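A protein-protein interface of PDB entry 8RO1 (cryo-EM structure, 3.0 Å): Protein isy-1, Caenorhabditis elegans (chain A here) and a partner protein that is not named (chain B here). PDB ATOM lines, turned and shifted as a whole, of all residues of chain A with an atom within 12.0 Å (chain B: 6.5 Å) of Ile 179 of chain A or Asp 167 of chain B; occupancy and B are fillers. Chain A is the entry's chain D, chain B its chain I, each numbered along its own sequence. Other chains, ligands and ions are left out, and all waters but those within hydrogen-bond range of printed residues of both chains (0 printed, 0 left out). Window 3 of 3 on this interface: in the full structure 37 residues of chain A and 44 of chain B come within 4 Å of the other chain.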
ATOM      1  N   ARG A 171      25.733  13.063  11.807  1.00  0.00           N
ATOM      2  CA  ARG A 171      26.351  11.753  11.617  1.00  0.00           C
ATOM      3  C   ARG A 171      25.420  10.608  11.998  1.00  0.00           C
ATOM      4  O   ARG A 171      25.777   9.445  11.787  1.00  0.00           O
ATOM      5  CB  ARG A 171      27.670  11.654  12.404  1.00  0.00           C
ATOM      6  CG  ARG A 171      27.575  11.235  13.880  1.00  0.00           C
ATOM      7  CD  ARG A 171      28.936  11.306  14.567  1.00  0.00           C
ATOM      8  NE  ARG A 171      29.326  12.658  14.949  1.00  0.00           N
ATOM      9  CZ  ARG A 171      30.507  12.995  15.454  1.00  0.00           C
ATOM     10  NH1 ARG A 171      30.701  14.242  15.874  1.00  0.00           N
ATOM     11  NH2 ARG A 171      31.513  12.134  15.515  1.00  0.00           N
ATOM     12  N   LEU A 172      24.249  10.906  12.559  1.00  0.00           N
ATOM     13  CA  LEU A 172      23.295   9.867  12.918  1.00  0.00           C
ATOM     14  C   LEU A 172      22.686   9.219  11.679  1.00  0.00           C
ATOM     15  O   LEU A 172      22.410   8.014  11.677  1.00  0.00           O
ATOM     16  CB  LEU A 172      22.209  10.457  13.818  1.00  0.00           C
ATOM     17  CG  LEU A 172      22.700  11.259  15.037  1.00  0.00           C
ATOM     18  CD1 LEU A 172      22.540  12.765  14.832  1.00  0.00           C
ATOM     19  CD2 LEU A 172      22.013  10.834  16.319  1.00  0.00           C
ATOM     20  N   ILE A 173      22.464  10.007  10.622  1.00  0.00           N
ATOM     21  CA  ILE A 173      21.734   9.504   9.454  1.00  0.00           C
ATOM     22  C   ILE A 173      22.452   8.346   8.764  1.00  0.00           C
ATOM     23  O   ILE A 173      21.783   7.360   8.415  1.00  0.00           O
ATOM     24  CB  ILE A 173      21.401  10.665   8.497  1.00  0.00           C
ATOM     25  CG1 ILE A 173      20.316  11.592   9.086  1.00  0.00           C
ATOM     26  CG2 ILE A 173      20.976  10.157   7.086  1.00  0.00           C
ATOM     27  CD1 ILE A 173      20.848  12.751   9.907  1.00  0.00           C
ATOM     28  N   PRO A 174      23.770   8.387   8.526  1.00  0.00           N
ATOM     29  CA  PRO A 174      24.401   7.221   7.886  1.00  0.00           C
ATOM     30  C   PRO A 174      24.339   5.950   8.709  1.00  0.00           C
ATOM     31  O   PRO A 174      24.264   4.859   8.130  1.00  0.00           O
ATOM     32  CB  PRO A 174      25.852   7.676   7.694  1.00  0.00           C
ATOM     33  CG  PRO A 174      25.762   9.125   7.564  1.00  0.00           C
ATOM     34  CD  PRO A 174      24.686   9.542   8.514  1.00  0.00           C
ATOM     35  N   LEU A 175      24.355   6.045  10.038  1.00  0.00           N
ATOM     36  CA  LEU A 175      24.138   4.850  10.847  1.00  0.00           C
ATOM     37  C   LEU A 175      22.704   4.359  10.706  1.00  0.00           C
ATOM     38  O   LEU A 175      22.462   3.156  10.557  1.00  0.00           O
ATOM     39  CB  LEU A 175      24.466   5.123  12.314  1.00  0.00           C
ATOM     40  CG  LEU A 175      25.938   5.102  12.741  1.00  0.00           C
ATOM     41  CD1 LEU A 175      26.742   6.260  12.159  1.00  0.00           C
ATOM     42  CD2 LEU A 175      26.047   5.082  14.260  1.00  0.00           C
ATOM     43  N   GLU A 176      21.745   5.286  10.764  1.00  0.00           N
ATOM     44  CA  GLU A 176      20.341   4.947  10.566  1.00  0.00           C
ATOM     45  C   GLU A 176      20.108   4.302   9.207  1.00  0.00           C
ATOM     46  O   GLU A 176      19.321   3.356   9.093  1.00  0.00           O
ATOM     47  CB  GLU A 176      19.486   6.203  10.728  1.00  0.00           C
ATOM     48  CG  GLU A 176      19.398   6.687  12.167  1.00  0.00           C
ATOM     49  CD  GLU A 176      18.502   7.897  12.335  1.00  0.00           C
ATOM     50  OE1 GLU A 176      18.693   8.891  11.604  1.00  0.00           O
ATOM     51  OE2 GLU A 176      17.604   7.857  13.203  1.00  0.00           O
ATOM     52  N   LYS A 177      20.756   4.830   8.164  1.00  0.00           N
ATOM     53  CA  LYS A 177      20.636   4.256   6.827  1.00  0.00           C
ATOM     54  C   LYS A 177      21.029   2.786   6.822  1.00  0.00           C
ATOM     55  O   LYS A 177      20.343   1.956   6.214  1.00  0.00           O
ATOM     56  CB  LYS A 177      21.483   5.066   5.838  1.00  0.00           C
ATOM     57  CG  LYS A 177      21.599   4.488   4.421  1.00  0.00           C
ATOM     58  CD  LYS A 177      20.259   4.465   3.708  1.00  0.00           C
ATOM     59  CE  LYS A 177      20.401   3.935   2.295  1.00  0.00           C
ATOM     60  NZ  LYS A 177      20.434   2.445   2.282  1.00  0.00           N
ATOM     61  N   LEU A 178      22.130   2.444   7.492  1.00  0.00           N
ATOM     62  CA  LEU A 178      22.622   1.072   7.449  1.00  0.00           C
ATOM     63  C   LEU A 178      21.649   0.116   8.126  1.00  0.00           C
ATOM     64  O   LEU A 178      21.441  -1.003   7.649  1.00  0.00           O
ATOM     65  CB  LEU A 178      23.998   0.990   8.111  1.00  0.00           C
ATOM     66  CG  LEU A 178      25.196   1.614   7.388  1.00  0.00           C
ATOM     67  CD1 LEU A 178      26.447   1.436   8.235  1.00  0.00           C
ATOM     68  CD2 LEU A 178      25.409   1.012   6.004  1.00  0.00           C
ATOM     69  N   ILE A 179      21.056   0.527   9.245  1.00  0.00           N
ATOM     70  CA  ILE A 179      20.042  -0.307   9.883  1.00  0.00           C
ATOM     71  C   ILE A 179      18.769  -0.329   9.046  1.00  0.00           C
ATOM     72  O   ILE A 179      18.085  -1.355   8.958  1.00  0.00           O
ATOM     73  CB  ILE A 179      19.768   0.189  11.318  1.00  0.00           C
ATOM     74  CG1 ILE A 179      21.055   0.238  12.165  1.00  0.00           C
ATOM     75  CG2 ILE A 179      18.723  -0.694  12.001  1.00  0.00           C
ATOM     76  CD1 ILE A 179      21.879  -1.053  12.223  1.00  0.00           C
ATOM     77  N   GLU A 180      18.422   0.808   8.442  1.00  0.00           N
ATOM     78  CA  GLU A 180      17.194   0.913   7.656  1.00  0.00           C
ATOM     79  C   GLU A 180      17.162  -0.054   6.475  1.00  0.00           C
ATOM     80  O   GLU A 180      16.114  -0.639   6.181  1.00  0.00           O
ATOM     81  CB  GLU A 180      17.032   2.354   7.168  1.00  0.00           C
ATOM     82  CG  GLU A 180      15.709   2.644   6.499  1.00  0.00           C
ATOM     83  CD  GLU A 180      15.452   4.127   6.334  1.00  0.00           C
ATOM     84  OE1 GLU A 180      15.054   4.779   7.322  1.00  0.00           O
ATOM     85  OE2 GLU A 180      15.649   4.643   5.214  1.00  0.00           O
ATOM     86  N   GLU A 181      18.299  -0.276   5.816  1.00  0.00           N
ATOM     87  CA  GLU A 181      18.294  -1.184   4.669  1.00  0.00           C
ATOM     88  C   GLU A 181      18.213  -2.648   5.085  1.00  0.00           C
ATOM     89  O   GLU A 181      17.513  -3.432   4.437  1.00  0.00           O
ATOM     90  CB  GLU A 181      19.513  -0.942   3.771  1.00  0.00           C
ATOM     91  CG  GLU A 181      20.882  -1.078   4.407  1.00  0.00           C
ATOM     92  CD  GLU A 181      21.965  -0.430   3.569  1.00  0.00           C
ATOM     93  OE1 GLU A 181      22.330  -1.003   2.521  1.00  0.00           O
ATOM     94  OE2 GLU A 181      22.449   0.651   3.961  1.00  0.00           O
ATOM     95  N   LYS A 182      18.897  -3.039   6.163  1.00  0.00           N
ATOM     96  CA  LYS A 182      18.755  -4.403   6.672  1.00  0.00           C
ATOM     97  C   LYS A 182      17.326  -4.698   7.110  1.00  0.00           C
ATOM     98  O   LYS A 182      16.875  -5.845   7.010  1.00  0.00           O
ATOM     99  CB  LYS A 182      19.731  -4.649   7.828  1.00  0.00           C
ATOM    100  CG  LYS A 182      21.229  -4.433   7.521  1.00  0.00           C
ATOM    101  CD  LYS A 182      21.729  -5.072   6.210  1.00  0.00           C
ATOM    102  CE  LYS A 182      21.673  -6.601   6.231  1.00  0.00           C
ATOM    103  NZ  LYS A 182      22.333  -7.221   7.419  1.00  0.00           N
ATOM    104  N   ASN A 183      16.603  -3.690   7.602  1.00  0.00           N
ATOM    105  CA  ASN A 183      15.180  -3.860   7.883  1.00  0.00           C
ATOM    106  C   ASN A 183      14.412  -4.221   6.620  1.00  0.00           C
ATOM    107  O   ASN A 183      13.564  -5.121   6.635  1.00  0.00           O
ATOM    108  CB  ASN A 183      14.597  -2.582   8.488  1.00  0.00           C
ATOM    109  CG  ASN A 183      14.615  -2.576  10.000  1.00  0.00           C
ATOM    110  OD1 ASN A 183      15.209  -3.440  10.640  1.00  0.00           O
ATOM    111  ND2 ASN A 183      13.946  -1.591  10.585  1.00  0.00           N
ATOM    112  N   ILE A 184      14.670  -3.502   5.526  1.00  0.00           N
ATOM    113  CA  ILE A 184      13.989  -3.768   4.261  1.00  0.00           C
ATOM    114  C   ILE A 184      14.254  -5.198   3.797  1.00  0.00           C
ATOM    115  O   ILE A 184      13.345  -5.889   3.322  1.00  0.00           O
ATOM    116  CB  ILE A 184      14.432  -2.723   3.213  1.00  0.00           C
ATOM    117  CG1 ILE A 184      13.881  -1.337   3.583  1.00  0.00           C
ATOM    118  CG2 ILE A 184      13.987  -3.113   1.778  1.00  0.00           C
ATOM    119  CD1 ILE A 184      14.546  -0.179   2.856  1.00  0.00           C
ATOM    120  N   GLU A 185      15.491  -5.672   3.945  1.00  0.00           N
ATOM    121  CA  GLU A 185      15.789  -7.064   3.622  1.00  0.00           C
ATOM    122  C   GLU A 185      15.127  -8.022   4.602  1.00  0.00           C
ATOM    123  O   GLU A 185      14.651  -9.094   4.206  1.00  0.00           O
ATOM    124  CB  GLU A 185      17.300  -7.305   3.610  1.00  0.00           C
ATOM    125  CG  GLU A 185      18.125  -6.336   2.773  1.00  0.00           C
ATOM    126  CD  GLU A 185      17.547  -6.091   1.397  1.00  0.00           C
ATOM    127  OE1 GLU A 185      17.371  -7.070   0.641  1.00  0.00           O
ATOM    128  OE2 GLU A 185      17.266  -4.918   1.073  1.00  0.00           O
ATOM    129  N   ARG A 186      15.070  -7.648   5.880  1.00  0.00           N
ATOM    130  CA  ARG A 186      14.485  -8.526   6.886  1.00  0.00           C
ATOM    131  C   ARG A 186      12.990  -8.720   6.669  1.00  0.00           C
ATOM    132  O   ARG A 186      12.481  -9.837   6.804  1.00  0.00           O
ATOM    133  CB  ARG A 186      14.748  -7.955   8.278  1.00  0.00           C
ATOM    134  CG  ARG A 186      14.582  -8.963   9.399  1.00  0.00           C
ATOM    135  CD  ARG A 186      13.737  -8.428  10.540  1.00  0.00           C
ATOM    136  NE  ARG A 186      12.355  -8.208  10.126  1.00  0.00           N
ATOM    137  CZ  ARG A 186      11.428  -9.153  10.020  1.00  0.00           C
ATOM    138  NH1 ARG A 186      10.200  -8.814   9.637  1.00  0.00           N
ATOM    139  NH2 ARG A 186      11.690 -10.425  10.282  1.00  0.00           N
ATOM    140  N   ILE A 187      12.271  -7.651   6.325  1.00  0.00           N
ATOM    141  CA  ILE A 187      10.840  -7.789   6.074  1.00  0.00           C
ATOM    142  C   ILE A 187      10.587  -8.541   4.772  1.00  0.00           C
ATOM    143  O   ILE A 187       9.607  -9.288   4.660  1.00  0.00           O
ATOM    144  CB  ILE A 187      10.156  -6.403   6.101  1.00  0.00           C
ATOM    145  CG1 ILE A 187      10.647  -5.484   4.969  1.00  0.00           C
ATOM    146  CG2 ILE A 187      10.332  -5.749   7.480  1.00  0.00           C
ATOM    147  CD1 ILE A 187       9.912  -4.155   4.886  1.00  0.00           C
ATOM    148  N   ASN A 188      11.451  -8.359   3.770  1.00  0.00           N
ATOM    149  CA  ASN A 188      11.290  -9.090   2.518  1.00  0.00           C
ATOM    150  C   ASN A 188      11.464 -10.589   2.720  1.00  0.00           C
ATOM    151  O   ASN A 188      10.729 -11.389   2.127  1.00  0.00           O
ATOM    152  CB  ASN A 188      12.292  -8.575   1.487  1.00  0.00           C
ATOM    153  CG  ASN A 188      11.919  -7.212   0.942  1.00  0.00           C
ATOM    154  OD1 ASN A 188      10.836  -6.694   1.211  1.00  0.00           O
ATOM    155  ND2 ASN A 188      12.819  -6.622   0.167  1.00  0.00           N
ATOM    156  N   GLY B 131       8.926   0.276   8.491  1.00  0.00           N
ATOM    157  CA  GLY B 131      10.286  -0.105   8.773  1.00  0.00           C
ATOM    158  C   GLY B 131      11.315   0.980   8.592  1.00  0.00           C
ATOM    159  O   GLY B 131      12.499   0.723   8.829  1.00  0.00           O
ATOM    160  N   ILE B 133      13.435   4.334   9.582  1.00  0.00           N
ATOM    161  CA  ILE B 133      13.971   4.806  10.850  1.00  0.00           C
ATOM    162  C   ILE B 133      14.253   6.299  10.821  1.00  0.00           C
ATOM    163  O   ILE B 133      13.953   7.009  11.785  1.00  0.00           O
ATOM    164  CB  ILE B 133      15.249   4.017  11.223  1.00  0.00           C
ATOM    165  CG1 ILE B 133      14.890   2.593  11.626  1.00  0.00           C
ATOM    166  CG2 ILE B 133      16.036   4.674  12.354  1.00  0.00           C
ATOM    167  CD1 ILE B 133      15.952   1.588  11.294  1.00  0.00           C
ATOM    168  N   LEU B 163      13.167   2.837  19.228  1.00  0.00           N
ATOM    169  CA  LEU B 163      14.622   2.980  19.198  1.00  0.00           C
ATOM    170  C   LEU B 163      15.344   1.809  19.854  1.00  0.00           C
ATOM    171  O   LEU B 163      16.317   1.282  19.310  1.00  0.00           O
ATOM    172  CB  LEU B 163      15.028   4.277  19.887  1.00  0.00           C
ATOM    173  CG  LEU B 163      14.727   5.587  19.176  1.00  0.00           C
ATOM    174  CD1 LEU B 163      15.098   6.756  20.035  1.00  0.00           C
ATOM    175  CD2 LEU B 163      15.498   5.666  17.875  1.00  0.00           C
ATOM    176  N   THR B 164      14.886   1.390  21.031  1.00  0.00           N
ATOM    177  CA  THR B 164      15.513   0.275  21.730  1.00  0.00           C
ATOM    178  C   THR B 164      15.230  -1.080  21.101  1.00  0.00           C
ATOM    179  O   THR B 164      15.793  -2.074  21.563  1.00  0.00           O
ATOM    180  CB  THR B 164      15.063   0.240  23.187  1.00  0.00           C
ATOM    181  OG1 THR B 164      13.646   0.063  23.260  1.00  0.00           O
ATOM    182  CG2 THR B 164      15.449   1.525  23.894  1.00  0.00           C
ATOM    183  N   SER B 165      14.377  -1.154  20.083  1.00  0.00           N
ATOM    184  CA  SER B 165      14.237  -2.378  19.305  1.00  0.00           C
ATOM    185  C   SER B 165      15.340  -2.564  18.270  1.00  0.00           C
ATOM    186  O   SER B 165      15.368  -3.618  17.626  1.00  0.00           O
ATOM    187  CB  SER B 165      12.890  -2.402  18.589  1.00  0.00           C
ATOM    188  OG  SER B 165      12.917  -1.567  17.447  1.00  0.00           O
ATOM    189  N   HIS B 166      16.233  -1.588  18.086  1.00  0.00           N
ATOM    190  CA  HIS B 166      17.223  -1.613  17.018  1.00  0.00           C
ATOM    191  C   HIS B 166      18.590  -1.267  17.583  1.00  0.00           C
ATOM    192  O   HIS B 166      18.716  -0.721  18.681  1.00  0.00           O
ATOM    193  CB  HIS B 166      16.891  -0.606  15.912  1.00  0.00           C
ATOM    194  CG  HIS B 166      15.616  -0.891  15.185  1.00  0.00           C
ATOM    195  ND1 HIS B 166      15.215  -2.166  14.852  1.00  0.00           N
ATOM    196  CD2 HIS B 166      14.654  -0.061  14.723  1.00  0.00           C
ATOM    197  CE1 HIS B 166      14.057  -2.109  14.218  1.00  0.00           C
ATOM    198  NE2 HIS B 166      13.695  -0.843  14.129  1.00  0.00           N
ATOM    199  N   ASP B 167      19.618  -1.571  16.793  1.00  0.00           N
ATOM    200  CA  ASP B 167      21.009  -1.309  17.162  1.00  0.00           C
ATOM    201  C   ASP B 167      21.400   0.117  16.778  1.00  0.00           C
ATOM    202  O   ASP B 167      22.277   0.356  15.949  1.00  0.00           O
ATOM    203  CB  ASP B 167      21.927  -2.334  16.507  1.00  0.00           C
ATOM    204  CG  ASP B 167      23.339  -2.307  17.072  1.00  0.00           C
ATOM    205  OD1 ASP B 167      23.548  -1.734  18.162  1.00  0.00           O
ATOM    206  OD2 ASP B 167      24.245  -2.864  16.419  1.00  0.00           O
ATOM    207  N   LEU B 168      20.733   1.072  17.424  1.00  0.00           N
ATOM    208  CA  LEU B 168      20.851   2.495  17.115  1.00  0.00           C
ATOM    209  C   LEU B 168      21.345   3.244  18.347  1.00  0.00           C
ATOM    210  O   LEU B 168      20.598   4.026  18.948  1.00  0.00           O
ATOM    211  CB  LEU B 168      19.500   3.041  16.661  1.00  0.00           C
ATOM    212  CG  LEU B 168      18.914   2.439  15.388  1.00  0.00           C
ATOM    213  CD1 LEU B 168      17.489   2.897  15.210  1.00  0.00           C
ATOM    214  CD2 LEU B 168      19.737   2.829  14.172  1.00  0.00           C
ATOM    215  N   PRO B 169      22.591   3.009  18.766  1.00  0.00           N
ATOM    216  CA  PRO B 169      23.043   3.537  20.058  1.00  0.00           C
ATOM    217  C   PRO B 169      23.121   5.053  20.102  1.00  0.00           C
ATOM    218  O   PRO B 169      22.700   5.673  21.082  1.00  0.00           O
ATOM    219  CB  PRO B 169      24.428   2.908  20.227  1.00  0.00           C
ATOM    220  CG  PRO B 169      24.876   2.603  18.871  1.00  0.00           C
ATOM    221  CD  PRO B 169      23.655   2.245  18.097  1.00  0.00           C
ATOM    222  N   GLU B 170      23.689   5.654  19.057  1.00  0.00           N
ATOM    223  CA  GLU B 170      23.930   7.093  19.071  1.00  0.00           C
ATOM    224  C   GLU B 170      22.629   7.889  19.072  1.00  0.00           C
ATOM    225  O   GLU B 170      22.527   8.908  19.764  1.00  0.00           O
ATOM    226  CB  GLU B 170      24.807   7.478  17.879  1.00  0.00           C
ATOM    227  CG  GLU B 170      25.181   8.956  17.792  1.00  0.00           C
ATOM    228  CD  GLU B 170      26.008   9.418  18.974  1.00  0.00           C
ATOM    229  OE1 GLU B 170      26.701   8.574  19.580  1.00  0.00           O
ATOM    230  OE2 GLU B 170      25.961  10.621  19.303  1.00  0.00           O
ATOM    231  N   THR B 172      19.593   6.743  20.123  1.00  0.00           N
ATOM    232  CA  THR B 172      18.851   6.433  21.338  1.00  0.00           C
ATOM    233  C   THR B 172      19.397   7.192  22.535  1.00  0.00           C
ATOM    234  O   THR B 172      18.633   7.589  23.417  1.00  0.00           O
ATOM    235  CB  THR B 172      18.877   4.925  21.598  1.00  0.00           C
ATOM    236  OG1 THR B 172      18.511   4.218  20.409  1.00  0.00           O
ATOM    237  CG2 THR B 172      17.890   4.556  22.675  1.00  0.00           C
ATOM    238  N   TYR B 193      19.770  -0.279  29.255  1.00  0.00           N
ATOM    239  CA  TYR B 193      19.948  -0.222  27.809  1.00  0.00           C
ATOM    240  C   TYR B 193      21.410  -0.007  27.447  1.00  0.00           C
ATOM    241  O   TYR B 193      21.954  -0.706  26.587  1.00  0.00           O
ATOM    242  CB  TYR B 193      19.082   0.881  27.204  1.00  0.00           C
ATOM    243  CG  TYR B 193      19.444   1.186  25.773  1.00  0.00           C
ATOM    244  CD1 TYR B 193      19.014   0.374  24.744  1.00  0.00           C
ATOM    245  CD2 TYR B 193      20.205   2.296  25.453  1.00  0.00           C
ATOM    246  CE1 TYR B 193      19.347   0.643  23.446  1.00  0.00           C
ATOM    247  CE2 TYR B 193      20.546   2.564  24.162  1.00  0.00           C
ATOM    248  CZ  TYR B 193      20.112   1.737  23.162  1.00  0.00           C
ATOM    249  OH  TYR B 193      20.447   2.009  21.858  1.00  0.00           O
ATOM    250  N   ARG B 197      23.924  -2.345  25.147  1.00  0.00           N
ATOM    251  CA  ARG B 197      24.573  -1.813  23.953  1.00  0.00           C
ATOM    252  C   ARG B 197      26.064  -1.556  24.136  1.00  0.00           C
ATOM    253  O   ARG B 197      26.685  -0.939  23.265  1.00  0.00           O
ATOM    254  CB  ARG B 197      23.838  -0.556  23.475  1.00  0.00           C
ATOM    255  CG  ARG B 197      22.856  -0.867  22.354  1.00  0.00           C
ATOM    256  CD  ARG B 197      21.776  -1.854  22.760  1.00  0.00           C
ATOM    257  NE  ARG B 197      20.824  -2.075  21.679  1.00  0.00           N
ATOM    258  CZ  ARG B 197      19.635  -2.647  21.815  1.00  0.00           C
ATOM    259  NH1 ARG B 197      18.845  -2.748  20.752  1.00  0.00           N
ATOM    260  NH2 ARG B 197      19.238  -3.170  22.966  1.00  0.00           N
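Ile 179 of chain A touches three residues of chain B.
Of chain A, only Ile 179 comes within 4 Å of Asp 167 of chain B.
No residue of chain A comes within 4 Å of Ser 165 of chain B.
Printed residues of chain A within 4 Å of His 166 of chain B: Asn 183.
Of chain A, only Ile 179 comes within 4 Å of Leu 168 of chain B.
No residue of chain A comes within 4 Å of Pro 169 of chain B.
Printed residues of chain B within 4 Å of Glu 176 of chain A: Ile 133 (3.6 Å).
Of the printed residues of chain B, Glu 180 of chain A touches Ile 133 (2.8 Å).
Printed residues of chain A within 4 Å of Ile 133 of chain B: Glu 176 (3.6 Å), Ile 179 (3.7 Å), Glu 180 (2.8 Å) and Asn 183 (3.8 Å).
Leu 163 of chain B touches none of the printed residues of chain A.
Lys 177 of chain A touches none of the printed residues of chain B.
The nearest residue of chain B that does not touch Ile 179 of chain A is His 166 of chain B (4.3 Å).
The nearest residue of chain A that does not touch Asp 167 of chain B is Leu 175 of chain A (6.1 Å).
O of His 166 of chain B is in hydrogen-bond range of NH1 of Arg 197 of chain B, at 2.9 Å.
A ring nitrogen (NE2) of His 166 of chain B lies close to the side-chain hydroxyl of Ser 165 of chain B.
The backbone carbonyl oxygen of Leu 168 of chain B is in hydrogen-bond range of the side-chain hydroxyl of Thr 172 of chain B (2.6 Å).
Of the 18 printed residues of chain A, 5 touch a printed residue of chain B.
Hydrophobic or aromatic side chains of chain A that line the printed part of chain B: Leu 172 and Ile 179.
Among the printed residues, 9 pairs touch across the chains.
Among the printed residues, no Asp or Glu carboxylate lies within 4 Å of a Lys or Arg side-chain nitrogen of the other chain.
The side-chain amide nitrogen (ND2) of Asn 183 of chain A sits at hydrogen-bond distance from the backbone carbonyl oxygen (O) of Gly 131 of chain B, 3.2 Å away.
The backbone NH (N) of Ile 133 of chain B sits at hydrogen-bond distance from the side-chain carboxylate (OE1) of Glu 180 of chain A, 2.8 Å away.
Among the printed residues, pairs that only touch across the chains: Leu 172 of chain A with Glu 170 of chain B (3.97 Å), Glu 176 of chain A with Ile 133 of chain B (3.6 Å), Ile 179 of chain A with Ile 133 of chain B (3.7 Å), Ile 179 of chain A with Asp 167 of chain B (3.98 Å), Ile 179 of chain A with Leu 168 of chain B (3.5 Å), Asn 183 of chain A with Ile 133 of chain B (3.8 Å) and Asn 183 of chain A with His 166 of chain B (3.6 Å).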
